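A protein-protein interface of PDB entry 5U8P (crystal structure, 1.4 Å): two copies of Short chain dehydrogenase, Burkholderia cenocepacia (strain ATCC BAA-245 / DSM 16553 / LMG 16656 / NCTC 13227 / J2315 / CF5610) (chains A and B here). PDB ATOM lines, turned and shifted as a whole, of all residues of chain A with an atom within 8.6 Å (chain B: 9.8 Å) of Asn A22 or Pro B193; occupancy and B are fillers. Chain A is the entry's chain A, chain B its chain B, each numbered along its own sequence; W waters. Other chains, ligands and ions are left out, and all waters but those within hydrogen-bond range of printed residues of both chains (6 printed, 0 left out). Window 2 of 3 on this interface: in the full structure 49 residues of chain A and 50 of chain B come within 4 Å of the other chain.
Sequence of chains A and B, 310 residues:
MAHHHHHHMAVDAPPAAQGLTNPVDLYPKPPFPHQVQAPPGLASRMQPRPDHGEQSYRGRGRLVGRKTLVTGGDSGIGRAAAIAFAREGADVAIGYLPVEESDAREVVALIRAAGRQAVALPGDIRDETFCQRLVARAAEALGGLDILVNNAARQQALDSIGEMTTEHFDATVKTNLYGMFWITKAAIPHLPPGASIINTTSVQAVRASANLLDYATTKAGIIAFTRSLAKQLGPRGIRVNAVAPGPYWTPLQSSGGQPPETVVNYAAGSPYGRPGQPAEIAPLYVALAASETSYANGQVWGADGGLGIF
The side-chain carboxylate (OE2) of Glu A280 lies within hydrogen-bond range of the side-chain hydroxyl (OG) of Ser B294. The backbone carbonyl oxygen (O) of Arg A274 is in hydrogen-bond range of the side-chain hydroxyl (OH) of Tyr B295. O of Gly A19 lies within hydrogen-bond range of OG of Ser B291. OH of Tyr A272 sits at hydrogen-bond distance from O of Ser B294 (2.8 Å).
OE2 of Glu A280 is in salt-bridge range of NH2 of Arg A274 (2.8 Å). The side-chain hydroxyl of Ser B196 lies within hydrogen-bond range of the guanidinium group of Arg B239 (3.5 Å). The backbone carbonyl oxygen of Ala B289 sits at hydrogen-bond distance from the guanidinium group of Arg B66 (3.2 Å).
Leu A20 touches Pro B193. Gly B194 touches Thr A21 (CA to O, 3.2 Å). CB of Pro B193 touches ND2 of Asn A22, 3.6 Å away. Asn A22 touches Gly B237 (OD1 to CA, 3.4 Å). Pro A23 touches Gly B237. Val A24 touches Gly B234 (CG2 to O, 3.2 Å). Val A24 touches Pro B235 (CG2 to O, 3.7 Å). Tyr A272 touches Gly B234 (CD1 to O, 3.4 Å). Tyr B295 touches Tyr A272 (CE1 to CD2, 3.7 Å). Glu B292 touches Glu A280.
Asn A22 touches two residues of chain B. Pro B193 touches just these residues of chain A: Leu A20 and Asn A22. Pro A23 touches just these residues of chain B: Gly B194 (3.9 Å), Gly B237 (3.4 Å) and Ser B294 (3.7 Å). Of chain B, only Gly B234 (3.2 Å), Pro B235 (3.7 Å) and Gly B237 (3.8 Å) come within 4 Å of Val A24. Gly B237 touches three residues of chain A. Printed residues of chain B within 4 Å of Arg A274: Tyr B295 (2.7 Å). Of the printed residues of chain A, Gly B194 touches Leu A20, Thr A21 and Pro A23. Of the printed residues of chain B, Gly A19 touches Ser B291. Of the printed residues of chain B, Glu A280 touches Glu B292 (3.7 Å), Ser B294 (2.6 Å) and Tyr B295 (3.6 Å). Asp A25 touches none of the printed residues of chain B.
Of the 12 printed residues of chain A, 9 touch a printed residue of chain B. Printed residues of chain B that touch a printed residue of chain A: Arg B66, Asp B146, Pro B193, Gly B194, Gly B234, Pro B235, Gly B237, Arg B239, Ser B291, Glu B292, Ser B294 and Tyr B295. Hydrophobic or aromatic side chains of chain B that line the printed part of chain A: Pro B193 and Tyr B295. Among the printed residues, no Asp or Glu carboxylate lies within 4 Å of a Lys or Arg side-chain nitrogen of the other chain.
No position is printed for both chains. Of the 22 pairs that touch across the chains among the printed residues, none has its exchanged pair printed and touching as well.
Water W6 lies within hydrogen-bond range of O of Glu A280, N of Tyr B295 and N of Ser B294. Water W2 lies within hydrogen-bond range of OG of Ser B291 (2.8 Å), O of Gly B194 (2.8 Å) and N of Thr A21 (3.2 Å). Water W1 lies within hydrogen-bond range of the side-chain hydroxyl (OG) of Ser B291, the guanidinium group (NH1) of Arg B66 and the backbone carbonyl oxygen (O) of Gly A19.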
ATOM      1  N   GLY A  19     -12.983 -23.678  -6.930  1.00  0.00           N
ATOM      2  CA  GLY A  19     -12.097 -22.989  -6.011  1.00  0.00           C
ATOM      3  C   GLY A  19     -10.690 -22.812  -6.545  1.00  0.00           C
ATOM      4  O   GLY A  19     -10.338 -23.343  -7.601  1.00  0.00           O
ATOM      5  N   LEU A  20      -9.882 -22.056  -5.808  1.00  0.00           N
ATOM      6  CA  LEU A  20      -8.494 -21.827  -6.170  1.00  0.00           C
ATOM      7  C   LEU A  20      -7.631 -22.942  -5.607  1.00  0.00           C
ATOM      8  O   LEU A  20      -7.831 -23.385  -4.475  1.00  0.00           O
ATOM      9  CB  LEU A  20      -8.026 -20.493  -5.593  1.00  0.00           C
ATOM     10  CG  LEU A  20      -8.840 -19.316  -6.121  1.00  0.00           C
ATOM     11  CD1 LEU A  20      -8.654 -18.114  -5.243  1.00  0.00           C
ATOM     12  CD2 LEU A  20      -8.425 -18.997  -7.538  1.00  0.00           C
ATOM     13  N   THR A  21      -6.665 -23.391  -6.402  1.00  0.00           N
ATOM     14  CA  THR A  21      -5.701 -24.396  -5.973  1.00  0.00           C
ATOM     15  C   THR A  21      -4.298 -23.886  -6.262  1.00  0.00           C
ATOM     16  O   THR A  21      -4.049 -23.327  -7.331  1.00  0.00           O
ATOM     17  CB  THR A  21      -5.924 -25.747  -6.689  1.00  0.00           C
ATOM     18  OG1 THR A  21      -5.710 -25.602  -8.102  1.00  0.00           O
ATOM     19  CG2 THR A  21      -7.343 -26.256  -6.440  1.00  0.00           C
ATOM     20  N   ASN A  22      -3.388 -24.071  -5.307  1.00  0.00           N
ATOM     21  CA  ASN A  22      -1.992 -23.658  -5.509  1.00  0.00           C
ATOM     22  C   ASN A  22      -1.321 -24.629  -6.469  1.00  0.00           C
ATOM     23  O   ASN A  22      -1.156 -25.808  -6.127  1.00  0.00           O
ATOM     24  CB  ASN A  22      -1.223 -23.624  -4.182  1.00  0.00           C
ATOM     25  CG  ASN A  22       0.171 -23.006  -4.323  1.00  0.00           C
ATOM     26  OD1 ASN A  22       0.717 -22.925  -5.412  1.00  0.00           O
ATOM     27  ND2 ASN A  22       0.743 -22.566  -3.213  1.00  0.00           N
ATOM     28  N   PRO A  23      -0.908 -24.190  -7.660  1.00  0.00           N
ATOM     29  CA  PRO A  23      -0.261 -25.124  -8.595  1.00  0.00           C
ATOM     30  C   PRO A  23       1.080 -25.652  -8.114  1.00  0.00           C
ATOM     31  O   PRO A  23       1.491 -26.724  -8.570  1.00  0.00           O
ATOM     32  CB  PRO A  23      -0.110 -24.300  -9.883  1.00  0.00           C
ATOM     33  CG  PRO A  23      -0.125 -22.867  -9.418  1.00  0.00           C
ATOM     34  CD  PRO A  23      -1.011 -22.823  -8.204  1.00  0.00           C
ATOM     35  N   VAL A  24       1.771 -24.954  -7.209  1.00  0.00           N
ATOM     36  CA  VAL A  24       3.141 -25.341  -6.861  1.00  0.00           C
ATOM     37  C   VAL A  24       3.188 -26.764  -6.325  1.00  0.00           C
ATOM     38  O   VAL A  24       3.993 -27.593  -6.771  1.00  0.00           O
ATOM     39  CB  VAL A  24       3.754 -24.349  -5.857  1.00  0.00           C
ATOM     40  CG1 VAL A  24       5.086 -24.898  -5.316  1.00  0.00           C
ATOM     41  CG2 VAL A  24       3.960 -22.977  -6.513  1.00  0.00           C
ATOM     42  N   ASP A  25       2.335 -27.067  -5.347  1.00  0.00           N
ATOM     43  CA  ASP A  25       2.402 -28.368  -4.687  1.00  0.00           C
ATOM     44  C   ASP A  25       1.238 -29.278  -5.065  1.00  0.00           C
ATOM     45  O   ASP A  25       0.930 -30.231  -4.342  1.00  0.00           O
ATOM     46  CB  ASP A  25       2.566 -28.224  -3.176  1.00  0.00           C
ATOM     47  CG  ASP A  25       1.464 -27.411  -2.549  1.00  0.00           C
ATOM     48  OD1 ASP A  25       0.561 -26.970  -3.285  1.00  0.00           O
ATOM     49  OD2 ASP A  25       1.496 -27.221  -1.314  1.00  0.00           O
ATOM     50  N   LEU A  26       0.630 -29.035  -6.224  1.00  0.00           N
ATOM     51  CA  LEU A  26      -0.475 -29.861  -6.688  1.00  0.00           C
ATOM     52  C   LEU A  26      -0.010 -31.248  -7.120  1.00  0.00           C
ATOM     53  O   LEU A  26      -0.808 -32.198  -7.106  1.00  0.00           O
ATOM     54  CB  LEU A  26      -1.151 -29.133  -7.850  1.00  0.00           C
ATOM     55  CG  LEU A  26      -2.494 -29.627  -8.381  1.00  0.00           C
ATOM     56  CD1 LEU A  26      -3.520 -29.758  -7.249  1.00  0.00           C
ATOM     57  CD2 LEU A  26      -3.008 -28.694  -9.481  1.00  0.00           C
ATOM     58  N   TYR A  27       1.267 -31.383  -7.475  1.00  0.00           N
ATOM     59  CA  TYR A  27       1.824 -32.613  -8.019  1.00  0.00           C
ATOM     60  C   TYR A  27       3.209 -32.858  -7.425  1.00  0.00           C
ATOM     61  O   TYR A  27       3.787 -31.951  -6.809  1.00  0.00           O
ATOM     62  CB  TYR A  27       1.905 -32.485  -9.544  1.00  0.00           C
ATOM     63  CG  TYR A  27       0.546 -32.405 -10.202  1.00  0.00           C
ATOM     64  CD1 TYR A  27       0.087 -31.208 -10.744  1.00  0.00           C
ATOM     65  CD2 TYR A  27      -0.275 -33.524 -10.291  1.00  0.00           C
ATOM     66  CE1 TYR A  27      -1.149 -31.117 -11.355  1.00  0.00           C
ATOM     67  CE2 TYR A  27      -1.528 -33.446 -10.912  1.00  0.00           C
ATOM     68  CZ  TYR A  27      -1.949 -32.236 -11.442  1.00  0.00           C
ATOM     69  OH  TYR A  27      -3.172 -32.149 -12.059  1.00  0.00           O
ATOM     70  N   TYR A 272       8.109 -23.553 -10.188  1.00  0.00           N
ATOM     71  CA  TYR A 272       7.399 -24.345  -9.182  1.00  0.00           C
ATOM     72  C   TYR A 272       8.297 -25.359  -8.487  1.00  0.00           C
ATOM     73  O   TYR A 272       7.887 -25.929  -7.469  1.00  0.00           O
ATOM     74  CB  TYR A 272       6.300 -25.200  -9.806  1.00  0.00           C
ATOM     75  CG  TYR A 272       5.143 -24.496 -10.454  1.00  0.00           C
ATOM     76  CD1 TYR A 272       4.791 -23.173 -10.142  1.00  0.00           C
ATOM     77  CD2 TYR A 272       4.347 -25.192 -11.344  1.00  0.00           C
ATOM     78  CE1 TYR A 272       3.696 -22.566 -10.752  1.00  0.00           C
ATOM     79  CE2 TYR A 272       3.274 -24.601 -11.953  1.00  0.00           C
ATOM     80  CZ  TYR A 272       2.955 -23.294 -11.676  1.00  0.00           C
ATOM     81  OH  TYR A 272       1.860 -22.766 -12.312  1.00  0.00           O
ATOM     82  N   ARG A 274       9.063 -28.311  -9.787  1.00  0.00           N
ATOM     83  CA  ARG A 274       8.581 -29.650 -10.103  1.00  0.00           C
ATOM     84  C   ARG A 274       8.316 -29.728 -11.597  1.00  0.00           C
ATOM     85  O   ARG A 274       8.051 -28.696 -12.231  1.00  0.00           O
ATOM     86  CB  ARG A 274       7.273 -29.959  -9.358  1.00  0.00           C
ATOM     87  CG  ARG A 274       6.095 -29.052  -9.762  1.00  0.00           C
ATOM     88  CD  ARG A 274       4.760 -29.626  -9.260  1.00  0.00           C
ATOM     89  NE  ARG A 274       3.613 -28.786  -9.613  1.00  0.00           N
ATOM     90  CZ  ARG A 274       2.963 -28.847 -10.781  1.00  0.00           C
ATOM     91  NH1 ARG A 274       3.349 -29.705 -11.724  1.00  0.00           N
ATOM     92  NH2 ARG A 274       1.915 -28.064 -11.005  1.00  0.00           N
ATOM     93  N   GLU A 280      -1.953 -31.828 -16.737  1.00  0.00           N
ATOM     94  CA  GLU A 280      -1.991 -30.368 -16.767  1.00  0.00           C
ATOM     95  C   GLU A 280      -2.016 -29.783 -18.169  1.00  0.00           C
ATOM     96  O   GLU A 280      -2.465 -28.639 -18.334  1.00  0.00           O
ATOM     97  CB  GLU A 280      -0.775 -29.805 -16.026  1.00  0.00           C
ATOM     98  CG  GLU A 280      -0.701 -30.275 -14.569  1.00  0.00           C
ATOM     99  CD  GLU A 280       0.478 -29.651 -13.831  1.00  0.00           C
ATOM    100  OE1 GLU A 280       1.579 -30.240 -13.857  1.00  0.00           O
ATOM    101  OE2 GLU A 280       0.311 -28.542 -13.271  1.00  0.00           O
ATOM    102  N   ARG B  66     -14.906 -17.120  -9.358  1.00  0.00           N
ATOM    103  CA  ARG B  66     -13.692 -16.331  -9.527  1.00  0.00           C
ATOM    104  C   ARG B  66     -14.028 -14.838  -9.499  1.00  0.00           C
ATOM    105  O   ARG B  66     -15.182 -14.426  -9.650  1.00  0.00           O
ATOM    106  CB  ARG B  66     -12.968 -16.727 -10.824  1.00  0.00           C
ATOM    107  CG  ARG B  66     -12.473 -18.183 -10.807  1.00  0.00           C
ATOM    108  CD  ARG B  66     -11.324 -18.417  -9.804  1.00  0.00           C
ATOM    109  NE  ARG B  66     -10.077 -17.741 -10.200  1.00  0.00           N
ATOM    110  CZ  ARG B  66      -9.118 -18.298 -10.935  1.00  0.00           C
ATOM    111  NH1 ARG B  66      -9.247 -19.536 -11.392  1.00  0.00           N
ATOM    112  NH2 ARG B  66      -8.025 -17.613 -11.221  1.00  0.00           N
ATOM    113  N   LEU B 145      -9.854 -10.730  -5.288  1.00  0.00           N
ATOM    114  CA  LEU B 145      -9.410 -10.606  -6.672  1.00  0.00           C
ATOM    115  C   LEU B 145      -8.513 -11.792  -6.995  1.00  0.00           C
ATOM    116  O   LEU B 145      -7.563 -12.064  -6.256  1.00  0.00           O
ATOM    117  CB  LEU B 145      -8.631  -9.295  -6.858  1.00  0.00           C
ATOM    118  CG  LEU B 145      -8.170  -8.986  -8.283  1.00  0.00           C
ATOM    119  CD1 LEU B 145      -9.375  -8.767  -9.189  1.00  0.00           C
ATOM    120  CD2 LEU B 145      -7.250  -7.775  -8.304  1.00  0.00           C
ATOM    121  N   ASP B 146      -8.810 -12.498  -8.100  1.00  0.00           N
ATOM    122  CA  ASP B 146      -7.984 -13.646  -8.461  1.00  0.00           C
ATOM    123  C   ASP B 146      -7.853 -13.891  -9.962  1.00  0.00           C
ATOM    124  O   ASP B 146      -7.186 -14.857 -10.350  1.00  0.00           O
ATOM    125  CB  ASP B 146      -8.449 -14.913  -7.701  1.00  0.00           C
ATOM    126  CG  ASP B 146      -9.943 -15.139  -7.819  1.00  0.00           C
ATOM    127  OD1 ASP B 146     -10.414 -15.275  -8.969  1.00  0.00           O
ATOM    128  OD2 ASP B 146     -10.642 -15.173  -6.771  1.00  0.00           O
ATOM    129  N   ILE B 147      -8.411 -13.033 -10.815  1.00  0.00           N
ATOM    130  CA  ILE B 147      -8.028 -12.960 -12.227  1.00  0.00           C
ATOM    131  C   ILE B 147      -7.855 -11.489 -12.561  1.00  0.00           C
ATOM    132  O   ILE B 147      -8.789 -10.700 -12.383  1.00  0.00           O
ATOM    133  CB  ILE B 147      -9.077 -13.573 -13.176  1.00  0.00           C
ATOM    134  CG1 ILE B 147      -9.373 -15.037 -12.815  1.00  0.00           C
ATOM    135  CG2 ILE B 147      -8.580 -13.466 -14.614  1.00  0.00           C
ATOM    136  CD1 ILE B 147     -10.554 -15.634 -13.601  1.00  0.00           C
ATOM    137  N   ILE B 188      -1.113  -7.468  -6.819  1.00  0.00           N
ATOM    138  CA  ILE B 188      -0.473  -8.675  -6.300  1.00  0.00           C
ATOM    139  C   ILE B 188      -0.769  -8.958  -4.833  1.00  0.00           C
ATOM    140  O   ILE B 188      -1.010 -10.130  -4.500  1.00  0.00           O
ATOM    141  CB  ILE B 188       1.003  -8.732  -6.719  1.00  0.00           C
ATOM    142  CG1 ILE B 188       1.069  -9.051  -8.226  1.00  0.00           C
ATOM    143  CG2 ILE B 188       1.775  -9.787  -5.909  1.00  0.00           C
ATOM    144  CD1 ILE B 188       2.348  -8.665  -8.901  1.00  0.00           C
ATOM    145  N   PRO B 189      -0.789  -7.980  -3.917  1.00  0.00           N
ATOM    146  CA  PRO B 189      -1.104  -8.316  -2.514  1.00  0.00           C
ATOM    147  C   PRO B 189      -2.478  -8.938  -2.308  1.00  0.00           C
ATOM    148  O   PRO B 189      -2.703  -9.568  -1.265  1.00  0.00           O
ATOM    149  CB  PRO B 189      -0.967  -6.969  -1.788  1.00  0.00           C
ATOM    150  CG  PRO B 189       0.033  -6.212  -2.633  1.00  0.00           C
ATOM    151  CD  PRO B 189      -0.362  -6.573  -4.044  1.00  0.00           C
ATOM    152  N   HIS B 190      -3.398  -8.795  -3.265  1.00  0.00           N
ATOM    153  CA  HIS B 190      -4.716  -9.418  -3.188  1.00  0.00           C
ATOM    154  C   HIS B 190      -4.758 -10.844  -3.736  1.00  0.00           C
ATOM    155  O   HIS B 190      -5.718 -11.572  -3.446  1.00  0.00           O
ATOM    156  CB  HIS B 190      -5.740  -8.601  -3.997  1.00  0.00           C
ATOM    157  CG  HIS B 190      -5.952  -7.209  -3.492  1.00  0.00           C
ATOM    158  ND1 HIS B 190      -6.859  -6.918  -2.493  1.00  0.00           N
ATOM    159  CD2 HIS B 190      -5.372  -6.031  -3.831  1.00  0.00           C
ATOM    160  CE1 HIS B 190      -6.835  -5.617  -2.250  1.00  0.00           C
ATOM    161  NE2 HIS B 190      -5.946  -5.058  -3.050  1.00  0.00           N
ATOM    162  N   LEU B 191      -3.771 -11.256  -4.535  1.00  0.00           N
ATOM    163  CA  LEU B 191      -3.912 -12.462  -5.352  1.00  0.00           C
ATOM    164  C   LEU B 191      -3.496 -13.695  -4.560  1.00  0.00           C
ATOM    165  O   LEU B 191      -2.317 -13.811  -4.191  1.00  0.00           O
ATOM    166  CB  LEU B 191      -3.060 -12.359  -6.616  1.00  0.00           C
ATOM    167  CG  LEU B 191      -3.377 -11.214  -7.578  1.00  0.00           C
ATOM    168  CD1 LEU B 191      -2.407 -11.241  -8.755  1.00  0.00           C
ATOM    169  CD2 LEU B 191      -4.814 -11.285  -8.101  1.00  0.00           C
ATOM    170  N   PRO B 192      -4.400 -14.640  -4.308  1.00  0.00           N
ATOM    171  CA  PRO B 192      -4.025 -15.848  -3.557  1.00  0.00           C
ATOM    172  C   PRO B 192      -3.355 -16.863  -4.464  1.00  0.00           C
ATOM    173  O   PRO B 192      -3.392 -16.735  -5.696  1.00  0.00           O
ATOM    174  CB  PRO B 192      -5.378 -16.385  -3.056  1.00  0.00           C
ATOM    175  CG  PRO B 192      -6.374 -15.275  -3.295  1.00  0.00           C
ATOM    176  CD  PRO B 192      -5.852 -14.579  -4.526  1.00  0.00           C
ATOM    177  N   PRO B 193      -2.718 -17.888  -3.899  1.00  0.00           N
ATOM    178  CA  PRO B 193      -2.235 -18.990  -4.739  1.00  0.00           C
ATOM    179  C   PRO B 193      -3.399 -19.548  -5.544  1.00  0.00           C
ATOM    180  O   PRO B 193      -4.514 -19.697  -5.038  1.00  0.00           O
ATOM    181  CB  PRO B 193      -1.708 -20.010  -3.720  1.00  0.00           C
ATOM    182  CG  PRO B 193      -1.365 -19.187  -2.518  1.00  0.00           C
ATOM    183  CD  PRO B 193      -2.402 -18.099  -2.474  1.00  0.00           C
ATOM    184  N   GLY B 194      -3.147 -19.804  -6.822  1.00  0.00           N
ATOM    185  CA  GLY B 194      -4.179 -20.206  -7.754  1.00  0.00           C
ATOM    186  C   GLY B 194      -4.687 -19.087  -8.641  1.00  0.00           C
ATOM    187  O   GLY B 194      -5.456 -19.354  -9.573  1.00  0.00           O
ATOM    188  N   ALA B 195      -4.269 -17.853  -8.391  1.00  0.00           N
ATOM    189  CA  ALA B 195      -4.714 -16.718  -9.190  1.00  0.00           C
ATOM    190  C   ALA B 195      -4.006 -16.678 -10.546  1.00  0.00           C
ATOM    191  O   ALA B 195      -2.980 -17.325 -10.768  1.00  0.00           O
ATOM    192  CB  ALA B 195      -4.452 -15.414  -8.446  1.00  0.00           C
ATOM    193  N   SER B 196      -4.552 -15.856 -11.450  1.00  0.00           N
ATOM    194  CA  SER B 196      -4.021 -15.708 -12.803  1.00  0.00           C
ATOM    195  C   SER B 196      -3.976 -14.245 -13.200  1.00  0.00           C
ATOM    196  O   SER B 196      -4.914 -13.487 -12.928  1.00  0.00           O
ATOM    197  CB  SER B 196      -4.936 -16.375 -13.827  1.00  0.00           C
ATOM    198  OG  SER B 196      -4.340 -17.514 -14.372  1.00  0.00           O
ATOM    199  N   LEU B 233       6.497 -14.782  -9.682  1.00  0.00           N
ATOM    200  CA  LEU B 233       5.285 -15.144  -8.944  1.00  0.00           C
ATOM    201  C   LEU B 233       4.950 -16.629  -8.992  1.00  0.00           C
ATOM    202  O   LEU B 233       4.195 -17.097  -8.139  1.00  0.00           O
ATOM    203  CB  LEU B 233       4.079 -14.352  -9.464  1.00  0.00           C
ATOM    204  CG  LEU B 233       4.160 -12.833  -9.369  1.00  0.00           C
ATOM    205  CD1 LEU B 233       2.847 -12.190  -9.822  1.00  0.00           C
ATOM    206  CD2 LEU B 233       4.530 -12.392  -7.953  1.00  0.00           C
ATOM    207  N   GLY B 234       5.479 -17.378  -9.959  1.00  0.00           N
ATOM    208  CA  GLY B 234       5.310 -18.817  -9.980  1.00  0.00           C
ATOM    209  C   GLY B 234       5.510 -19.489  -8.629  1.00  0.00           C
ATOM    210  O   GLY B 234       4.710 -20.333  -8.214  1.00  0.00           O
ATOM    211  N   PRO B 235       6.576 -19.132  -7.910  1.00  0.00           N
ATOM    212  CA  PRO B 235       6.801 -19.755  -6.593  1.00  0.00           C
ATOM    213  C   PRO B 235       5.712 -19.482  -5.562  1.00  0.00           C
ATOM    214  O   PRO B 235       5.556 -20.286  -4.630  1.00  0.00           O
ATOM    215  CB  PRO B 235       8.172 -19.197  -6.170  1.00  0.00           C
ATOM    216  CG  PRO B 235       8.847 -18.881  -7.455  1.00  0.00           C
ATOM    217  CD  PRO B 235       7.763 -18.366  -8.343  1.00  0.00           C
ATOM    218  N   ARG B 236       4.955 -18.390  -5.693  1.00  0.00           N
ATOM    219  CA  ARG B 236       3.796 -18.039  -4.885  1.00  0.00           C
ATOM    220  C   ARG B 236       2.500 -18.613  -5.437  1.00  0.00           C
ATOM    221  O   ARG B 236       1.423 -18.279  -4.923  1.00  0.00           O
ATOM    222  CB  ARG B 236       3.646 -16.514  -4.830  1.00  0.00           C
ATOM    223  CG  ARG B 236       4.584 -15.804  -3.872  1.00  0.00           C
ATOM    224  CD  ARG B 236       4.744 -14.339  -4.262  1.00  0.00           C
ATOM    225  NE  ARG B 236       3.555 -13.536  -3.984  1.00  0.00           N
ATOM    226  CZ  ARG B 236       3.562 -12.421  -3.260  1.00  0.00           C
ATOM    227  NH1 ARG B 236       2.436 -11.754  -3.054  1.00  0.00           N
ATOM    228  NH2 ARG B 236       4.698 -11.970  -2.745  1.00  0.00           N
ATOM    229  N   GLY B 237       2.565 -19.404  -6.500  1.00  0.00           N
ATOM    230  CA  GLY B 237       1.371 -20.013  -7.047  1.00  0.00           C
ATOM    231  C   GLY B 237       0.513 -19.121  -7.908  1.00  0.00           C
ATOM    232  O   GLY B 237      -0.657 -19.444  -8.116  1.00  0.00           O
ATOM    233  N   ILE B 238       1.048 -18.016  -8.424  1.00  0.00           N
ATOM    234  CA  ILE B 238       0.307 -17.115  -9.305  1.00  0.00           C
ATOM    235  C   ILE B 238       0.866 -17.269 -10.708  1.00  0.00           C
ATOM    236  O   ILE B 238       2.077 -17.144 -10.909  1.00  0.00           O
ATOM    237  CB  ILE B 238       0.434 -15.651  -8.849  1.00  0.00           C
ATOM    238  CG1 ILE B 238      -0.128 -15.461  -7.441  1.00  0.00           C
ATOM    239  CG2 ILE B 238      -0.273 -14.710  -9.830  1.00  0.00           C
ATOM    240  CD1 ILE B 238       0.339 -14.171  -6.796  1.00  0.00           C
ATOM    241  N   ARG B 239      -0.003 -17.532 -11.680  1.00  0.00           N
ATOM    242  CA  ARG B 239       0.410 -17.703 -13.068  1.00  0.00           C
ATOM    243  C   ARG B 239       0.213 -16.403 -13.839  1.00  0.00           C
ATOM    244  O   ARG B 239      -0.772 -15.693 -13.632  1.00  0.00           O
ATOM    245  CB  ARG B 239      -0.384 -18.840 -13.724  1.00  0.00           C
ATOM    246  CG  ARG B 239      -0.067 -20.180 -13.089  1.00  0.00           C
ATOM    247  CD  ARG B 239      -0.714 -21.357 -13.809  1.00  0.00           C
ATOM    248  NE  ARG B 239      -2.175 -21.346 -13.772  1.00  0.00           N
ATOM    249  CZ  ARG B 239      -2.953 -20.946 -14.768  1.00  0.00           C
ATOM    250  NH1 ARG B 239      -2.433 -20.508 -15.910  1.00  0.00           N
ATOM    251  NH2 ARG B 239      -4.267 -20.977 -14.622  1.00  0.00           N
ATOM    252  N   ALA B 289      -7.057 -18.738 -17.584  1.00  0.00           N
ATOM    253  CA  ALA B 289      -7.458 -18.475 -16.205  1.00  0.00           C
ATOM    254  C   ALA B 289      -7.850 -19.746 -15.454  1.00  0.00           C
ATOM    255  O   ALA B 289      -7.730 -19.793 -14.224  1.00  0.00           O
ATOM    256  CB  ALA B 289      -8.632 -17.495 -16.199  1.00  0.00           C
ATOM    257  N   SER B 291      -8.315 -23.114 -13.411  1.00  0.00           N
ATOM    258  CA  SER B 291      -7.402 -23.744 -12.457  1.00  0.00           C
ATOM    259  C   SER B 291      -6.743 -25.002 -13.020  1.00  0.00           C
ATOM    260  O   SER B 291      -5.624 -25.350 -12.615  1.00  0.00           O
ATOM    261  CB  SER B 291      -8.151 -24.072 -11.160  1.00  0.00           C
ATOM    262  OG  SER B 291      -8.727 -22.907 -10.581  1.00  0.00           O
ATOM    263  N   GLU B 292      -7.410 -25.705 -13.941  1.00  0.00           N
ATOM    264  CA  GLU B 292      -6.855 -26.939 -14.509  1.00  0.00           C
ATOM    265  C   GLU B 292      -5.655 -26.698 -15.425  1.00  0.00           C
ATOM    266  O   GLU B 292      -4.917 -27.647 -15.696  1.00  0.00           O
ATOM    267  CB  GLU B 292      -7.928 -27.717 -15.284  1.00  0.00           C
ATOM    268  CG  GLU B 292      -8.444 -26.953 -16.506  1.00  0.00           C
ATOM    269  CD  GLU B 292      -9.342 -27.772 -17.406  1.00  0.00           C
ATOM    270  OE1 GLU B 292      -9.613 -28.952 -17.088  1.00  0.00           O
ATOM    271  OE2 GLU B 292      -9.779 -27.221 -18.444  1.00  0.00           O
ATOM    272  N   THR B 293      -5.440 -25.467 -15.900  1.00  0.00           N
ATOM    273  CA  THR B 293      -4.359 -25.171 -16.844  1.00  0.00           C
ATOM    274  C   THR B 293      -3.087 -24.792 -16.077  1.00  0.00           C
ATOM    275  O   THR B 293      -2.467 -23.737 -16.267  1.00  0.00           O
ATOM    276  CB  THR B 293      -4.806 -24.081 -17.821  1.00  0.00           C
ATOM    277  OG1 THR B 293      -6.165 -24.323 -18.227  1.00  0.00           O
ATOM    278  CG2 THR B 293      -3.898 -24.028 -19.074  1.00  0.00           C
ATOM    279  N   SER B 294      -2.691 -25.704 -15.189  1.00  0.00           N
ATOM    280  CA  SER B 294      -1.854 -25.341 -14.050  1.00  0.00           C
ATOM    281  C   SER B 294      -0.361 -25.291 -14.361  1.00  0.00           C
ATOM    282  O   SER B 294       0.402 -24.833 -13.503  1.00  0.00           O
ATOM    283  CB  SER B 294      -2.153 -26.270 -12.860  1.00  0.00           C
ATOM    284  OG  SER B 294      -2.129 -27.640 -13.256  1.00  0.00           O
ATOM    285  N   TYR B 295       0.072 -25.726 -15.549  1.00  0.00           N
ATOM    286  CA  TYR B 295       1.474 -25.639 -15.961  1.00  0.00           C
ATOM    287  C   TYR B 295       1.683 -24.643 -17.095  1.00  0.00           C
ATOM    288  O   TYR B 295       2.742 -24.651 -17.734  1.00  0.00           O
ATOM    289  CB  TYR B 295       2.052 -27.029 -16.290  1.00  0.00           C
ATOM    290  CG  TYR B 295       3.515 -27.250 -15.880  1.00  0.00           C
ATOM    291  CD1 TYR B 295       3.878 -27.296 -14.529  1.00  0.00           C
ATOM    292  CD2 TYR B 295       4.523 -27.451 -16.841  1.00  0.00           C
ATOM    293  CE1 TYR B 295       5.201 -27.532 -14.145  1.00  0.00           C
ATOM    294  CE2 TYR B 295       5.852 -27.681 -16.469  1.00  0.00           C
ATOM    295  CZ  TYR B 295       6.188 -27.712 -15.122  1.00  0.00           C
ATOM    296  OH  TYR B 295       7.503 -27.956 -14.758  1.00  0.00           O
HETATM  297  O   HOH W   1     -11.255 -21.681 -10.410  1.00  0.00           O
HETATM  298  O   HOH W   2      -6.499 -21.980  -9.255  1.00  0.00           O
HETATM  299  O   HOH W   3      -4.504 -24.071 -10.332  1.00  0.00           O
HETATM  300  O   HOH W   4      -4.118 -29.604 -12.784  1.00  0.00           O
HETATM  301  O   HOH W   5       3.560 -21.507  -2.965  1.00  0.00           O
HETATM  302  O   HOH W   6      -1.066 -26.355 -18.148  1.00  0.00           O
